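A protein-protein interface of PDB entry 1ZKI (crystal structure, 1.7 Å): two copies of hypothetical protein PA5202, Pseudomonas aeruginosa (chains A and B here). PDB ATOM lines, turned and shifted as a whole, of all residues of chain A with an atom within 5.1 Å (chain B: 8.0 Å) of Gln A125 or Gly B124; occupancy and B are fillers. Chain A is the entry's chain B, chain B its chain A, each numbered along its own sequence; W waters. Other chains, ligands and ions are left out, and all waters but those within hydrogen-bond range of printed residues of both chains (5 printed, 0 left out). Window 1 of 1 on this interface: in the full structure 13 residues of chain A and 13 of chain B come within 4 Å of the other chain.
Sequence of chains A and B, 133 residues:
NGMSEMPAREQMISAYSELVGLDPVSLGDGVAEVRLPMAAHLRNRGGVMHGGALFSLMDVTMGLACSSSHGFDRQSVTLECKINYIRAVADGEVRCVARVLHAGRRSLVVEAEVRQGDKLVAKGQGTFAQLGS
Water W3 lies within hydrogen-bond range of OE1 of Gln A125 (2.7 Å), NZ of Lys B123 (2.7 Å) and OE1 of Glu A111 (3.2 Å). Water W1 lies within hydrogen-bond range of the side-chain amide nitrogen (NE2) of Gln B125 (2.7 Å), the side-chain amino group (NZ) of Lys A123 (2.7 Å) and the side-chain carboxylate (OE1) of Glu B111 (3.3 Å). Water W5 lies within hydrogen-bond range of OE1 of Glu B111 and OE1 of Glu A111.
Lys A82 touches its own counterpart, Lys B82. Lys A82 touches Gln B125, and with the chains exchanged Gln A125 touches Lys B82. Lys A123 touches Gln B125, and with the chains exchanged Gln A125 touches Lys B123. Gly A124 touches Gln B125, and with the chains exchanged Gln A125 touches Gly B124. Of the 16 pairs that touch across the chains among the printed residues, 10 have their exchanged pair printed and touching as well.
Gln A125 touches four residues of chain B. Gly A124 touches one residue of chain B. Of the printed residues of chain A, Lys B123 touches Glu A111 (2.7 Å) and Gln A125 (2.9 Å). Printed residues of chain B within 4 Å of Thr A127: Asn B84. Of the printed residues of chain B, Glu A80 touches Lys B82 (2.7 Å). Of the printed residues of chain A, Ile B86 touches Val A109 (3.98 Å). Gly A126 touches none of the printed residues of chain B. The nearest printed residue of chain A that does not touch Gly B124 is Lys A82 (6.7 Å).
CB of Lys B82 touches CE of Lys A82, 3.8 Å away. CE of Lys A82 touches O of Gln B125, 3.5 Å away. CG2 of Val A109 touches OD1 of Asn B84 (3.7 Å). Ile B86 touches Val A109 (CG1 to CG2, 3.98 Å). Glu B111 touches Glu A111 (OE1 to OE1, 3.6 Å). CG of Lys A123 touches CD1 of Leu B101, 3.6 Å away. Gln B125 touches Gly A124. Lys B82 touches Gln A125 (CE to O, 3.5 Å). Gly B124 touches Gln A125 (CA to OE1, 3.5 Å).
The side-chain amino group (NZ) of Lys B82 sits close to the side-chain amide nitrogen (ND2) of Asn B84 (2.8 Å). The backbone NH (N) of Lys B82 lies within hydrogen-bond range of the backbone carbonyl oxygen (O) of Gln B125 (2.9 Å). The backbone NH (N) of Gly B124 is in hydrogen-bond range of the backbone carbonyl oxygen (O) of Ala B112, 2.9 Å away.
Printed residues of chain B that touch a printed residue of chain A: Lys B82, Asn B84, Ile B86, Leu B101, Glu B111, Lys B123, Gly B124 and Gln B125. Hydrophobic or aromatic side chains of chain B that line the printed part of chain A: Ile B86 and Leu B101. Along chain B the printed residues that touch a printed residue of chain A span positions 82 to 125. Printed residues of chain A that touch a printed residue of chain B: Glu A80, Lys A82, Val A109, Glu A111, Lys A123, Gly A124, Gln A125 and Thr A127. Among the printed residues, Asp or Glu carboxylates within 4 Å of a Lys or Arg side-chain nitrogen of the other chain: Glu A80 with Lys B82 (2.7 Å), Glu A111 with Lys B123 (2.7 Å) and Lys A123 with Glu B111 (2.6 Å).
OE1 of Glu A80 is in salt-bridge range of NZ of Lys B82 (2.7 Å). The side-chain amide nitrogen of Gln A125 lies close to the side-chain amide nitrogen of Asn B84. The side-chain amide oxygen (OD1) of Asn B84 sits at hydrogen-bond distance from the side-chain hydroxyl (OG1) of Thr A127, 2.9 Å away. The side-chain carboxylate of Glu B111 is in salt-bridge range of the side-chain amino group of Lys A123, at 2.6 Å. The side-chain amino group (NZ) of Lys B123 is in salt-bridge range of the side-chain carboxylate (OE1) of Glu A111, 2.7 Å away. The backbone carbonyl oxygen of Lys B123 sits at hydrogen-bond distance from the side-chain amide nitrogen of Gln A125 (2.9 Å). O of Lys A123 sits close to OE1 of Gln B125 (2.9 Å).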
ATOM      1  N   MET A  58     -14.227  12.104  22.083  1.00  0.00           N
ATOM      2  CA  MET A  58     -14.493  10.778  21.542  1.00  0.00           C
ATOM      3  C   MET A  58     -13.279  10.216  20.789  1.00  0.00           C
ATOM      4  O   MET A  58     -12.908   9.068  20.986  1.00  0.00           O
ATOM      5  CB  MET A  58     -15.741  10.791  20.654  1.00  0.00           C
ATOM      6  CG  MET A  58     -16.091   9.411  20.163  1.00  0.00           C
ATOM      7  SD  MET A  58     -17.755   9.544  19.173  1.00  0.00           S
ATOM      8  CE  MET A  58     -18.951   9.976  20.623  1.00  0.00           C
ATOM      9  N   MET A  62     -11.351   6.783  21.818  1.00  0.00           N
ATOM     10  CA  MET A  62     -11.260   5.681  20.842  1.00  0.00           C
ATOM     11  C   MET A  62      -9.795   5.286  20.614  1.00  0.00           C
ATOM     12  O   MET A  62      -9.473   4.100  20.516  1.00  0.00           O
ATOM     13  CB  MET A  62     -11.928   6.088  19.522  1.00  0.00           C
ATOM     14  CG  MET A  62     -13.431   6.136  19.613  1.00  0.00           C
ATOM     15  SD  MET A  62     -14.025   6.867  17.860  1.00  0.00           S
ATOM     16  CE  MET A  62     -15.904   6.155  17.896  1.00  0.00           C
ATOM     17  N   GLU A  80     -11.223   7.357   9.950  1.00  0.00           N
ATOM     18  CA  GLU A  80     -12.493   8.062   9.801  1.00  0.00           C
ATOM     19  C   GLU A  80     -13.326   7.883  11.068  1.00  0.00           C
ATOM     20  O   GLU A  80     -13.113   6.932  11.838  1.00  0.00           O
ATOM     21  CB  GLU A  80     -13.264   7.553   8.561  1.00  0.00           C
ATOM     22  CG  GLU A  80     -13.759   6.095   8.700  1.00  0.00           C
ATOM     23  CD  GLU A  80     -15.082   5.980   9.474  1.00  0.00           C
ATOM     24  OE1 GLU A  80     -15.261   4.955  10.167  1.00  0.00           O
ATOM     25  OE2 GLU A  80     -15.949   6.881   9.376  1.00  0.00           O
ATOM     26  N   CYS A  81     -14.289   8.778  11.284  1.00  0.00           N
ATOM     27  CA  CYS A  81     -15.161   8.643  12.433  1.00  0.00           C
ATOM     28  C   CYS A  81     -16.460   9.373  12.144  1.00  0.00           C
ATOM     29  O   CYS A  81     -16.466  10.355  11.370  1.00  0.00           O
ATOM     30  CB  CYS A  81     -14.495   9.219  13.670  1.00  0.00           C
ATOM     31  SG  CYS A  81     -15.423   8.879  15.192  1.00  0.00           S
ATOM     32  N   LYS A  82     -17.544   8.877  12.745  1.00  0.00           N
ATOM     33  CA  LYS A  82     -18.882   9.444  12.553  1.00  0.00           C
ATOM     34  C   LYS A  82     -19.497   9.612  13.935  1.00  0.00           C
ATOM     35  O   LYS A  82     -19.425   8.688  14.768  1.00  0.00           O
ATOM     36  CB  LYS A  82     -19.712   8.508  11.682  1.00  0.00           C
ATOM     37  CG  LYS A  82     -21.177   8.940  11.404  1.00  0.00           C
ATOM     38  CD  LYS A  82     -22.148   8.278  12.370  1.00  0.00           C
ATOM     39  CE  LYS A  82     -23.549   8.261  11.776  1.00  0.00           C
ATOM     40  NZ  LYS A  82     -24.218   9.601  11.885  1.00  0.00           N
ATOM     41  N   VAL A 109     -12.185  -1.345  14.372  1.00  0.00           N
ATOM     42  CA  VAL A 109     -13.475  -0.645  14.425  1.00  0.00           C
ATOM     43  C   VAL A 109     -13.759  -0.395  15.888  1.00  0.00           C
ATOM     44  O   VAL A 109     -13.626  -1.304  16.707  1.00  0.00           O
ATOM     45  CB  VAL A 109     -14.597  -1.488  13.792  1.00  0.00           C
ATOM     46  CG1 VAL A 109     -15.927  -0.696  13.780  1.00  0.00           C
ATOM     47  CG2 VAL A 109     -14.206  -1.867  12.375  1.00  0.00           C
ATOM     48  N   VAL A 110     -14.155   0.831  16.210  1.00  0.00           N
ATOM     49  CA  VAL A 110     -14.343   1.261  17.600  1.00  0.00           C
ATOM     50  C   VAL A 110     -15.648   2.036  17.684  1.00  0.00           C
ATOM     51  O   VAL A 110     -16.001   2.783  16.751  1.00  0.00           O
ATOM     52  CB  VAL A 110     -13.188   2.187  18.100  1.00  0.00           C
ATOM     53  CG1 VAL A 110     -13.277   2.424  19.616  1.00  0.00           C
ATOM     54  CG2 VAL A 110     -11.864   1.605  17.762  1.00  0.00           C
ATOM     55  N   GLU A 111     -16.378   1.844  18.784  1.00  0.00           N
ATOM     56  CA  GLU A 111     -17.543   2.686  19.044  1.00  0.00           C
ATOM     57  C   GLU A 111     -17.359   3.436  20.366  1.00  0.00           C
ATOM     58  O   GLU A 111     -16.521   3.072  21.192  1.00  0.00           O
ATOM     59  CB  GLU A 111     -18.823   1.861  19.082  1.00  0.00           C
ATOM     60  CG  GLU A 111     -18.891   0.928  20.289  1.00  0.00           C
ATOM     61  CD  GLU A 111     -20.255   0.230  20.467  1.00  0.00           C
ATOM     62  OE1 GLU A 111     -21.237   0.576  19.771  1.00  0.00           O
ATOM     63  OE2 GLU A 111     -20.323  -0.662  21.332  1.00  0.00           O
ATOM     64  N   ALA A 112     -18.118   4.498  20.559  1.00  0.00           N
ATOM     65  CA  ALA A 112     -17.992   5.251  21.803  1.00  0.00           C
ATOM     66  C   ALA A 112     -19.269   5.970  22.137  1.00  0.00           C
ATOM     67  O   ALA A 112     -20.045   6.323  21.244  1.00  0.00           O
ATOM     68  CB  ALA A 112     -16.859   6.252  21.714  1.00  0.00           C
ATOM     69  N   LYS A 123     -22.944   9.724  20.462  1.00  0.00           N
ATOM     70  CA  LYS A 123     -22.606   8.334  20.156  1.00  0.00           C
ATOM     71  C   LYS A 123     -21.830   8.355  18.862  1.00  0.00           C
ATOM     72  O   LYS A 123     -22.143   9.147  17.962  1.00  0.00           O
ATOM     73  CB  LYS A 123     -23.879   7.493  19.994  1.00  0.00           C
ATOM     74  CG  LYS A 123     -23.602   5.994  19.666  1.00  0.00           C
ATOM     75  CD  LYS A 123     -23.222   5.217  20.925  1.00  0.00           C
ATOM     76  CE  LYS A 123     -22.374   3.939  20.647  1.00  0.00           C
ATOM     77  NZ  LYS A 123     -23.265   2.818  20.338  1.00  0.00           N
ATOM     78  N   GLY A 124     -20.802   7.517  18.766  1.00  0.00           N
ATOM     79  CA  GLY A 124     -20.022   7.483  17.534  1.00  0.00           C
ATOM     80  C   GLY A 124     -19.401   6.142  17.215  1.00  0.00           C
ATOM     81  O   GLY A 124     -19.353   5.238  18.052  1.00  0.00           O
ATOM     82  N   GLN A 125     -18.921   6.037  15.982  1.00  0.00           N
ATOM     83  CA  GLN A 125     -18.296   4.828  15.493  1.00  0.00           C
ATOM     84  C   GLN A 125     -17.232   5.244  14.509  1.00  0.00           C
ATOM     85  O   GLN A 125     -17.470   6.135  13.688  1.00  0.00           O
ATOM     86  CB  GLN A 125     -19.365   3.982  14.806  1.00  0.00           C
ATOM     87  CG  GLN A 125     -18.896   2.677  14.202  1.00  0.00           C
ATOM     88  CD  GLN A 125     -20.079   1.933  13.568  1.00  0.00           C
ATOM     89  OE1 GLN A 125     -21.157   1.840  14.167  1.00  0.00           O
ATOM     90  NE2 GLN A 125     -19.884   1.413  12.362  1.00  0.00           N
ATOM     91  N   GLY A 126     -16.066   4.612  14.573  1.00  0.00           N
ATOM     92  CA  GLY A 126     -15.001   4.994  13.664  1.00  0.00           C
ATOM     93  C   GLY A 126     -14.061   3.855  13.359  1.00  0.00           C
ATOM     94  O   GLY A 126     -14.186   2.753  13.927  1.00  0.00           O
ATOM     95  N   THR A 127     -13.138   4.124  12.438  1.00  0.00           N
ATOM     96  CA  THR A 127     -12.201   3.104  11.952  1.00  0.00           C
ATOM     97  C   THR A 127     -10.790   3.644  12.142  1.00  0.00           C
ATOM     98  O   THR A 127     -10.521   4.826  11.848  1.00  0.00           O
ATOM     99  CB  THR A 127     -12.439   2.851  10.453  1.00  0.00           C
ATOM    100  OG1 THR A 127     -13.845   2.709  10.210  1.00  0.00           O
ATOM    101  CG2 THR A 127     -11.696   1.602   9.969  1.00  0.00           C
ATOM    102  N   PHE B  55     -26.262  -3.734   4.234  1.00  0.00           N
ATOM    103  CA  PHE B  55     -26.782  -2.421   4.561  1.00  0.00           C
ATOM    104  C   PHE B  55     -28.314  -2.406   4.498  1.00  0.00           C
ATOM    105  O   PHE B  55     -28.956  -1.801   5.350  1.00  0.00           O
ATOM    106  CB  PHE B  55     -26.200  -1.354   3.642  1.00  0.00           C
ATOM    107  CG  PHE B  55     -26.752   0.006   3.905  1.00  0.00           C
ATOM    108  CD1 PHE B  55     -26.087   0.879   4.770  1.00  0.00           C
ATOM    109  CD2 PHE B  55     -27.961   0.398   3.322  1.00  0.00           C
ATOM    110  CE1 PHE B  55     -26.606   2.150   5.036  1.00  0.00           C
ATOM    111  CE2 PHE B  55     -28.500   1.661   3.575  1.00  0.00           C
ATOM    112  CZ  PHE B  55     -27.819   2.547   4.431  1.00  0.00           C
ATOM    113  N   MET B  58     -29.656  -3.781   7.543  1.00  0.00           N
ATOM    114  CA  MET B  58     -29.527  -2.829   8.633  1.00  0.00           C
ATOM    115  C   MET B  58     -30.568  -1.700   8.561  1.00  0.00           C
ATOM    116  O   MET B  58     -31.223  -1.397   9.549  1.00  0.00           O
ATOM    117  CB  MET B  58     -28.112  -2.240   8.680  1.00  0.00           C
ATOM    118  CG  MET B  58     -27.927  -1.310   9.863  1.00  0.00           C
ATOM    119  SD  MET B  58     -26.064  -0.826   9.979  1.00  0.00           S
ATOM    120  CE  MET B  58     -25.386  -2.601  10.449  1.00  0.00           C
ATOM    121  N   MET B  62     -33.374  -0.988  11.423  1.00  0.00           N
ATOM    122  CA  MET B  62     -33.424   0.327  12.067  1.00  0.00           C
ATOM    123  C   MET B  62     -34.795   0.991  11.903  1.00  0.00           C
ATOM    124  O   MET B  62     -35.313   1.548  12.852  1.00  0.00           O
ATOM    125  CB  MET B  62     -32.318   1.230  11.529  1.00  0.00           C
ATOM    126  CG  MET B  62     -30.932   0.819  11.964  1.00  0.00           C
ATOM    127  SD  MET B  62     -29.698   2.090  11.032  1.00  0.00           S
ATOM    128  CE  MET B  62     -28.139   1.825  12.166  1.00  0.00           C
ATOM    129  N   CYS B  81     -27.113   7.162   7.262  1.00  0.00           N
ATOM    130  CA  CYS B  81     -26.634   5.983   7.992  1.00  0.00           C
ATOM    131  C   CYS B  81     -25.181   5.752   7.651  1.00  0.00           C
ATOM    132  O   CYS B  81     -24.740   6.087   6.545  1.00  0.00           O
ATOM    133  CB  CYS B  81     -27.459   4.752   7.604  1.00  0.00           C
ATOM    134  SG  CYS B  81     -27.163   3.349   8.691  1.00  0.00           S
ATOM    135  N   LYS B  82     -24.455   5.142   8.585  1.00  0.00           N
ATOM    136  CA  LYS B  82     -23.040   4.833   8.417  1.00  0.00           C
ATOM    137  C   LYS B  82     -22.850   3.409   8.883  1.00  0.00           C
ATOM    138  O   LYS B  82     -23.331   3.056   9.948  1.00  0.00           O
ATOM    139  CB  LYS B  82     -22.201   5.775   9.283  1.00  0.00           C
ATOM    140  CG  LYS B  82     -20.672   5.558   9.209  1.00  0.00           C
ATOM    141  CD  LYS B  82     -20.139   4.768  10.404  1.00  0.00           C
ATOM    142  CE  LYS B  82     -18.640   5.048  10.608  1.00  0.00           C
ATOM    143  NZ  LYS B  82     -17.805   4.341   9.629  1.00  0.00           N
ATOM    144  N   ILE B  83     -22.132   2.616   8.094  1.00  0.00           N
ATOM    145  CA  ILE B  83     -21.933   1.193   8.395  1.00  0.00           C
ATOM    146  C   ILE B  83     -20.451   0.848   8.315  1.00  0.00           C
ATOM    147  O   ILE B  83     -19.738   1.395   7.470  1.00  0.00           O
ATOM    148  CB  ILE B  83     -22.747   0.299   7.374  1.00  0.00           C
ATOM    149  CG1 ILE B  83     -22.678  -1.187   7.749  1.00  0.00           C
ATOM    150  CG2 ILE B  83     -22.277   0.507   5.897  1.00  0.00           C
ATOM    151  CD1 ILE B  83     -23.705  -2.033   7.014  1.00  0.00           C
ATOM    152  N   ASN B  84     -19.988  -0.051   9.192  1.00  0.00           N
ATOM    153  CA  ASN B  84     -18.667  -0.678   9.068  1.00  0.00           C
ATOM    154  C   ASN B  84     -18.861  -2.142   8.778  1.00  0.00           C
ATOM    155  O   ASN B  84     -19.689  -2.794   9.413  1.00  0.00           O
ATOM    156  CB  ASN B  84     -17.865  -0.572  10.361  1.00  0.00           C
ATOM    157  CG  ASN B  84     -17.007   0.652  10.401  1.00  0.00           C
ATOM    158  OD1 ASN B  84     -15.794   0.603  10.099  1.00  0.00           O
ATOM    159  ND2 ASN B  84     -17.616   1.757  10.739  1.00  0.00           N
ATOM    160  N   TYR B  85     -18.075  -2.651   7.841  1.00  0.00           N
ATOM    161  CA  TYR B  85     -18.086  -4.076   7.503  1.00  0.00           C
ATOM    162  C   TYR B  85     -16.912  -4.735   8.183  1.00  0.00           C
ATOM    163  O   TYR B  85     -15.756  -4.322   7.997  1.00  0.00           O
ATOM    164  CB  TYR B  85     -17.969  -4.244   5.989  1.00  0.00           C
ATOM    165  CG  TYR B  85     -19.138  -3.627   5.268  1.00  0.00           C
ATOM    166  CD1 TYR B  85     -20.373  -4.277   5.250  1.00  0.00           C
ATOM    167  CD2 TYR B  85     -19.014  -2.397   4.623  1.00  0.00           C
ATOM    168  CE1 TYR B  85     -21.477  -3.710   4.597  1.00  0.00           C
ATOM    169  CE2 TYR B  85     -20.112  -1.818   3.953  1.00  0.00           C
ATOM    170  CZ  TYR B  85     -21.335  -2.484   3.958  1.00  0.00           C
ATOM    171  OH  TYR B  85     -22.410  -1.932   3.296  1.00  0.00           O
ATOM    172  N   ILE B  86     -17.195  -5.765   8.959  1.00  0.00           N
ATOM    173  CA  ILE B  86     -16.139  -6.329   9.803  1.00  0.00           C
ATOM    174  C   ILE B  86     -15.617  -7.640   9.246  1.00  0.00           C
ATOM    175  O   ILE B  86     -14.396  -7.840   9.139  1.00  0.00           O
ATOM    176  CB  ILE B  86     -16.606  -6.418  11.273  1.00  0.00           C
ATOM    177  CG1 ILE B  86     -16.625  -4.986  11.846  1.00  0.00           C
ATOM    178  CG2 ILE B  86     -15.687  -7.350  12.088  1.00  0.00           C
ATOM    179  CD1 ILE B  86     -17.522  -4.789  13.023  1.00  0.00           C
ATOM    180  N   CYS B  96     -29.800  -9.129  12.315  1.00  0.00           N
ATOM    181  CA  CYS B  96     -29.554  -7.735  12.660  1.00  0.00           C
ATOM    182  C   CYS B  96     -30.445  -7.356  13.829  1.00  0.00           C
ATOM    183  O   CYS B  96     -31.656  -7.625  13.813  1.00  0.00           O
ATOM    184  CB  CYS B  96     -29.831  -6.839  11.469  1.00  0.00           C
ATOM    185  SG  CYS B  96     -29.550  -5.072  11.852  1.00  0.00           S
ATOM    186  N   VAL B  97     -29.840  -6.758  14.854  1.00  0.00           N
ATOM    187  CA  VAL B  97     -30.600  -6.170  15.957  1.00  0.00           C
ATOM    188  C   VAL B  97     -30.324  -4.668  15.967  1.00  0.00           C
ATOM    189  O   VAL B  97     -29.155  -4.249  15.981  1.00  0.00           O
ATOM    190  CB  VAL B  97     -30.218  -6.796  17.316  1.00  0.00           C
ATOM    191  CG1 VAL B  97     -30.982  -6.106  18.455  1.00  0.00           C
ATOM    192  CG2 VAL B  97     -30.499  -8.304  17.289  1.00  0.00           C
ATOM    193  N   ALA B  98     -31.394  -3.872  15.939  1.00  0.00           N
ATOM    194  CA  ALA B  98     -31.277  -2.425  15.961  1.00  0.00           C
ATOM    195  C   ALA B  98     -31.953  -1.900  17.224  1.00  0.00           C
ATOM    196  O   ALA B  98     -32.944  -2.474  17.695  1.00  0.00           O
ATOM    197  CB  ALA B  98     -31.914  -1.803  14.719  1.00  0.00           C
ATOM    198  N   ARG B  99     -31.401  -0.811  17.762  1.00  0.00           N
ATOM    199  CA  ARG B  99     -31.856  -0.243  19.015  1.00  0.00           C
ATOM    200  C   ARG B  99     -31.889   1.274  18.903  1.00  0.00           C
ATOM    201  O   ARG B  99     -30.874   1.892  18.567  1.00  0.00           O
ATOM    202  CB  ARG B  99     -30.887  -0.659  20.123  1.00  0.00           C
ATOM    203  CG  ARG B  99     -31.325  -0.289  21.521  1.00  0.00           C
ATOM    204  CD  ARG B  99     -30.346  -0.896  22.555  1.00  0.00           C
ATOM    205  NE  ARG B  99     -30.257  -2.353  22.388  1.00  0.00           N
ATOM    206  CZ  ARG B  99     -31.079  -3.247  22.949  1.00  0.00           C
ATOM    207  NH1 ARG B  99     -32.071  -2.860  23.754  1.00  0.00           N
ATOM    208  NH2 ARG B  99     -30.906  -4.545  22.705  1.00  0.00           N
ATOM    209  N   LEU B 101     -31.445   4.740  20.226  1.00  0.00           N
ATOM    210  CA  LEU B 101     -30.624   5.333  21.300  1.00  0.00           C
ATOM    211  C   LEU B 101     -31.224   6.636  21.805  1.00  0.00           C
ATOM    212  O   LEU B 101     -30.991   7.041  22.951  1.00  0.00           O
ATOM    213  CB  LEU B 101     -29.219   5.637  20.785  1.00  0.00           C
ATOM    214  CG  LEU B 101     -28.412   4.413  20.344  1.00  0.00           C
ATOM    215  CD1 LEU B 101     -27.031   4.794  19.830  1.00  0.00           C
ATOM    216  CD2 LEU B 101     -28.305   3.411  21.466  1.00  0.00           C
ATOM    217  N   VAL B 110     -30.310   5.740  15.968  1.00  0.00           N
ATOM    218  CA  VAL B 110     -30.437   4.284  16.071  1.00  0.00           C
ATOM    219  C   VAL B 110     -29.093   3.635  15.782  1.00  0.00           C
ATOM    220  O   VAL B 110     -28.336   4.144  14.940  1.00  0.00           O
ATOM    221  CB  VAL B 110     -31.482   3.721  15.047  1.00  0.00           C
ATOM    222  CG1 VAL B 110     -31.782   2.239  15.313  1.00  0.00           C
ATOM    223  CG2 VAL B 110     -32.765   4.523  15.076  1.00  0.00           C
ATOM    224  N   GLU B 111     -28.765   2.563  16.515  1.00  0.00           N
ATOM    225  CA  GLU B 111     -27.577   1.774  16.198  1.00  0.00           C
ATOM    226  C   GLU B 111     -28.022   0.376  15.824  1.00  0.00           C
ATOM    227  O   GLU B 111     -29.157  -0.016  16.132  1.00  0.00           O
ATOM    228  CB  GLU B 111     -26.594   1.726  17.376  1.00  0.00           C
ATOM    229  CG  GLU B 111     -27.099   0.955  18.582  1.00  0.00           C
ATOM    230  CD  GLU B 111     -26.009   0.704  19.655  1.00  0.00           C
ATOM    231  OE1 GLU B 111     -24.808   0.916  19.378  1.00  0.00           O
ATOM    232  OE2 GLU B 111     -26.368   0.286  20.775  1.00  0.00           O
ATOM    233  N   ALA B 112     -27.154  -0.374  15.152  1.00  0.00           N
ATOM    234  CA  ALA B 112     -27.495  -1.753  14.790  1.00  0.00           C
ATOM    235  C   ALA B 112     -26.242  -2.584  14.642  1.00  0.00           C
ATOM    236  O   ALA B 112     -25.167  -2.050  14.362  1.00  0.00           O
ATOM    237  CB  ALA B 112     -28.340  -1.804  13.510  1.00  0.00           C
ATOM    238  N   GLU B 113     -26.367  -3.886  14.882  1.00  0.00           N
ATOM    239  CA  GLU B 113     -25.276  -4.810  14.640  1.00  0.00           C
ATOM    240  C   GLU B 113     -25.818  -6.000  13.865  1.00  0.00           C
ATOM    241  O   GLU B 113     -26.990  -6.374  14.021  1.00  0.00           O
ATOM    242  CB  GLU B 113     -24.605  -5.276  15.945  1.00  0.00           C
ATOM    243  CG  GLU B 113     -25.519  -6.011  16.878  1.00  0.00           C
ATOM    244  CD  GLU B 113     -24.772  -6.693  18.029  1.00  0.00           C
ATOM    245  OE1 GLU B 113     -25.376  -7.576  18.674  1.00  0.00           O
ATOM    246  OE2 GLU B 113     -23.588  -6.368  18.262  1.00  0.00           O
ATOM    247  N   VAL B 114     -24.984  -6.539  12.989  1.00  0.00           N
ATOM    248  CA  VAL B 114     -25.309  -7.752  12.252  1.00  0.00           C
ATOM    249  C   VAL B 114     -24.355  -8.823  12.740  1.00  0.00           C
ATOM    250  O   VAL B 114     -23.142  -8.582  12.837  1.00  0.00           O
ATOM    251  CB  VAL B 114     -25.131  -7.557  10.735  1.00  0.00           C
ATOM    252  CG1 VAL B 114     -25.459  -8.860   9.973  1.00  0.00           C
ATOM    253  CG2 VAL B 114     -26.011  -6.382  10.246  1.00  0.00           C
ATOM    254  N   LEU B 120     -19.244 -11.069  14.772  1.00  0.00           N
ATOM    255  CA  LEU B 120     -19.710  -9.727  14.414  1.00  0.00           C
ATOM    256  C   LEU B 120     -19.416  -9.470  12.948  1.00  0.00           C
ATOM    257  O   LEU B 120     -18.252  -9.506  12.519  1.00  0.00           O
ATOM    258  CB  LEU B 120     -19.057  -8.652  15.294  1.00  0.00           C
ATOM    259  CG  LEU B 120     -19.489  -7.210  15.031  1.00  0.00           C
ATOM    260  CD1 LEU B 120     -20.978  -6.994  15.233  1.00  0.00           C
ATOM    261  CD2 LEU B 120     -18.683  -6.234  15.925  1.00  0.00           C
ATOM    262  N   ALA B 122     -21.205  -6.769  10.937  1.00  0.00           N
ATOM    263  CA  ALA B 122     -21.252  -5.324  10.598  1.00  0.00           C
ATOM    264  C   ALA B 122     -21.840  -4.544  11.764  1.00  0.00           C
ATOM    265  O   ALA B 122     -22.503  -5.112  12.628  1.00  0.00           O
ATOM    266  CB  ALA B 122     -22.081  -5.092   9.326  1.00  0.00           C
ATOM    267  N   LYS B 123     -21.561  -3.249  11.799  1.00  0.00           N
ATOM    268  CA  LYS B 123     -22.062  -2.393  12.872  1.00  0.00           C
ATOM    269  C   LYS B 123     -22.371  -1.058  12.225  1.00  0.00           C
ATOM    270  O   LYS B 123     -21.641  -0.613  11.328  1.00  0.00           O
ATOM    271  CB  LYS B 123     -20.998  -2.191  13.954  1.00  0.00           C
ATOM    272  CG  LYS B 123     -21.474  -1.333  15.145  1.00  0.00           C
ATOM    273  CD  LYS B 123     -22.280  -2.198  16.126  1.00  0.00           C
ATOM    274  CE  LYS B 123     -23.380  -1.420  16.855  1.00  0.00           C
ATOM    275  NZ  LYS B 123     -22.888  -0.586  17.948  1.00  0.00           N
ATOM    276  N   GLY B 124     -23.466  -0.429  12.641  1.00  0.00           N
ATOM    277  CA  GLY B 124     -23.782   0.906  12.094  1.00  0.00           C
ATOM    278  C   GLY B 124     -24.583   1.795  13.010  1.00  0.00           C
ATOM    279  O   GLY B 124     -25.045   1.353  14.070  1.00  0.00           O
ATOM    280  N   GLN B 125     -24.760   3.037  12.566  1.00  0.00           N
ATOM    281  CA  GLN B 125     -25.435   4.076  13.328  1.00  0.00           C
ATOM    282  C   GLN B 125     -26.063   4.996  12.313  1.00  0.00           C
ATOM    283  O   GLN B 125     -25.431   5.319  11.309  1.00  0.00           O
ATOM    284  CB  GLN B 125     -24.385   4.843  14.139  1.00  0.00           C
ATOM    285  CG  GLN B 125     -24.914   5.891  15.082  1.00  0.00           C
ATOM    286  CD  GLN B 125     -23.783   6.574  15.849  1.00  0.00           C
ATOM    287  OE1 GLN B 125     -23.645   7.805  15.814  1.00  0.00           O
ATOM    288  NE2 GLN B 125     -22.950   5.773  16.514  1.00  0.00           N
ATOM    289  N   GLY B 126     -27.303   5.401  12.560  1.00  0.00           N
ATOM    290  CA  GLY B 126     -28.017   6.291  11.623  1.00  0.00           C
ATOM    291  C   GLY B 126     -28.990   7.222  12.314  1.00  0.00           C
ATOM    292  O   GLY B 126     -29.232   7.113  13.536  1.00  0.00           O
HETATM  293  O   HOH W   1     -23.401   3.391  17.652  1.00  0.00           O
HETATM  294  O   HOH W   2     -22.093  -2.478  19.689  1.00  0.00           O
HETATM  295  O   HOH W   3     -21.759   1.522  16.742  1.00  0.00           O
HETATM  296  O   HOH W   4     -24.912   2.336  22.385  1.00  0.00           O
HETATM  297  O   HOH W   5     -23.418  -0.590  21.598  1.00  0.00           O
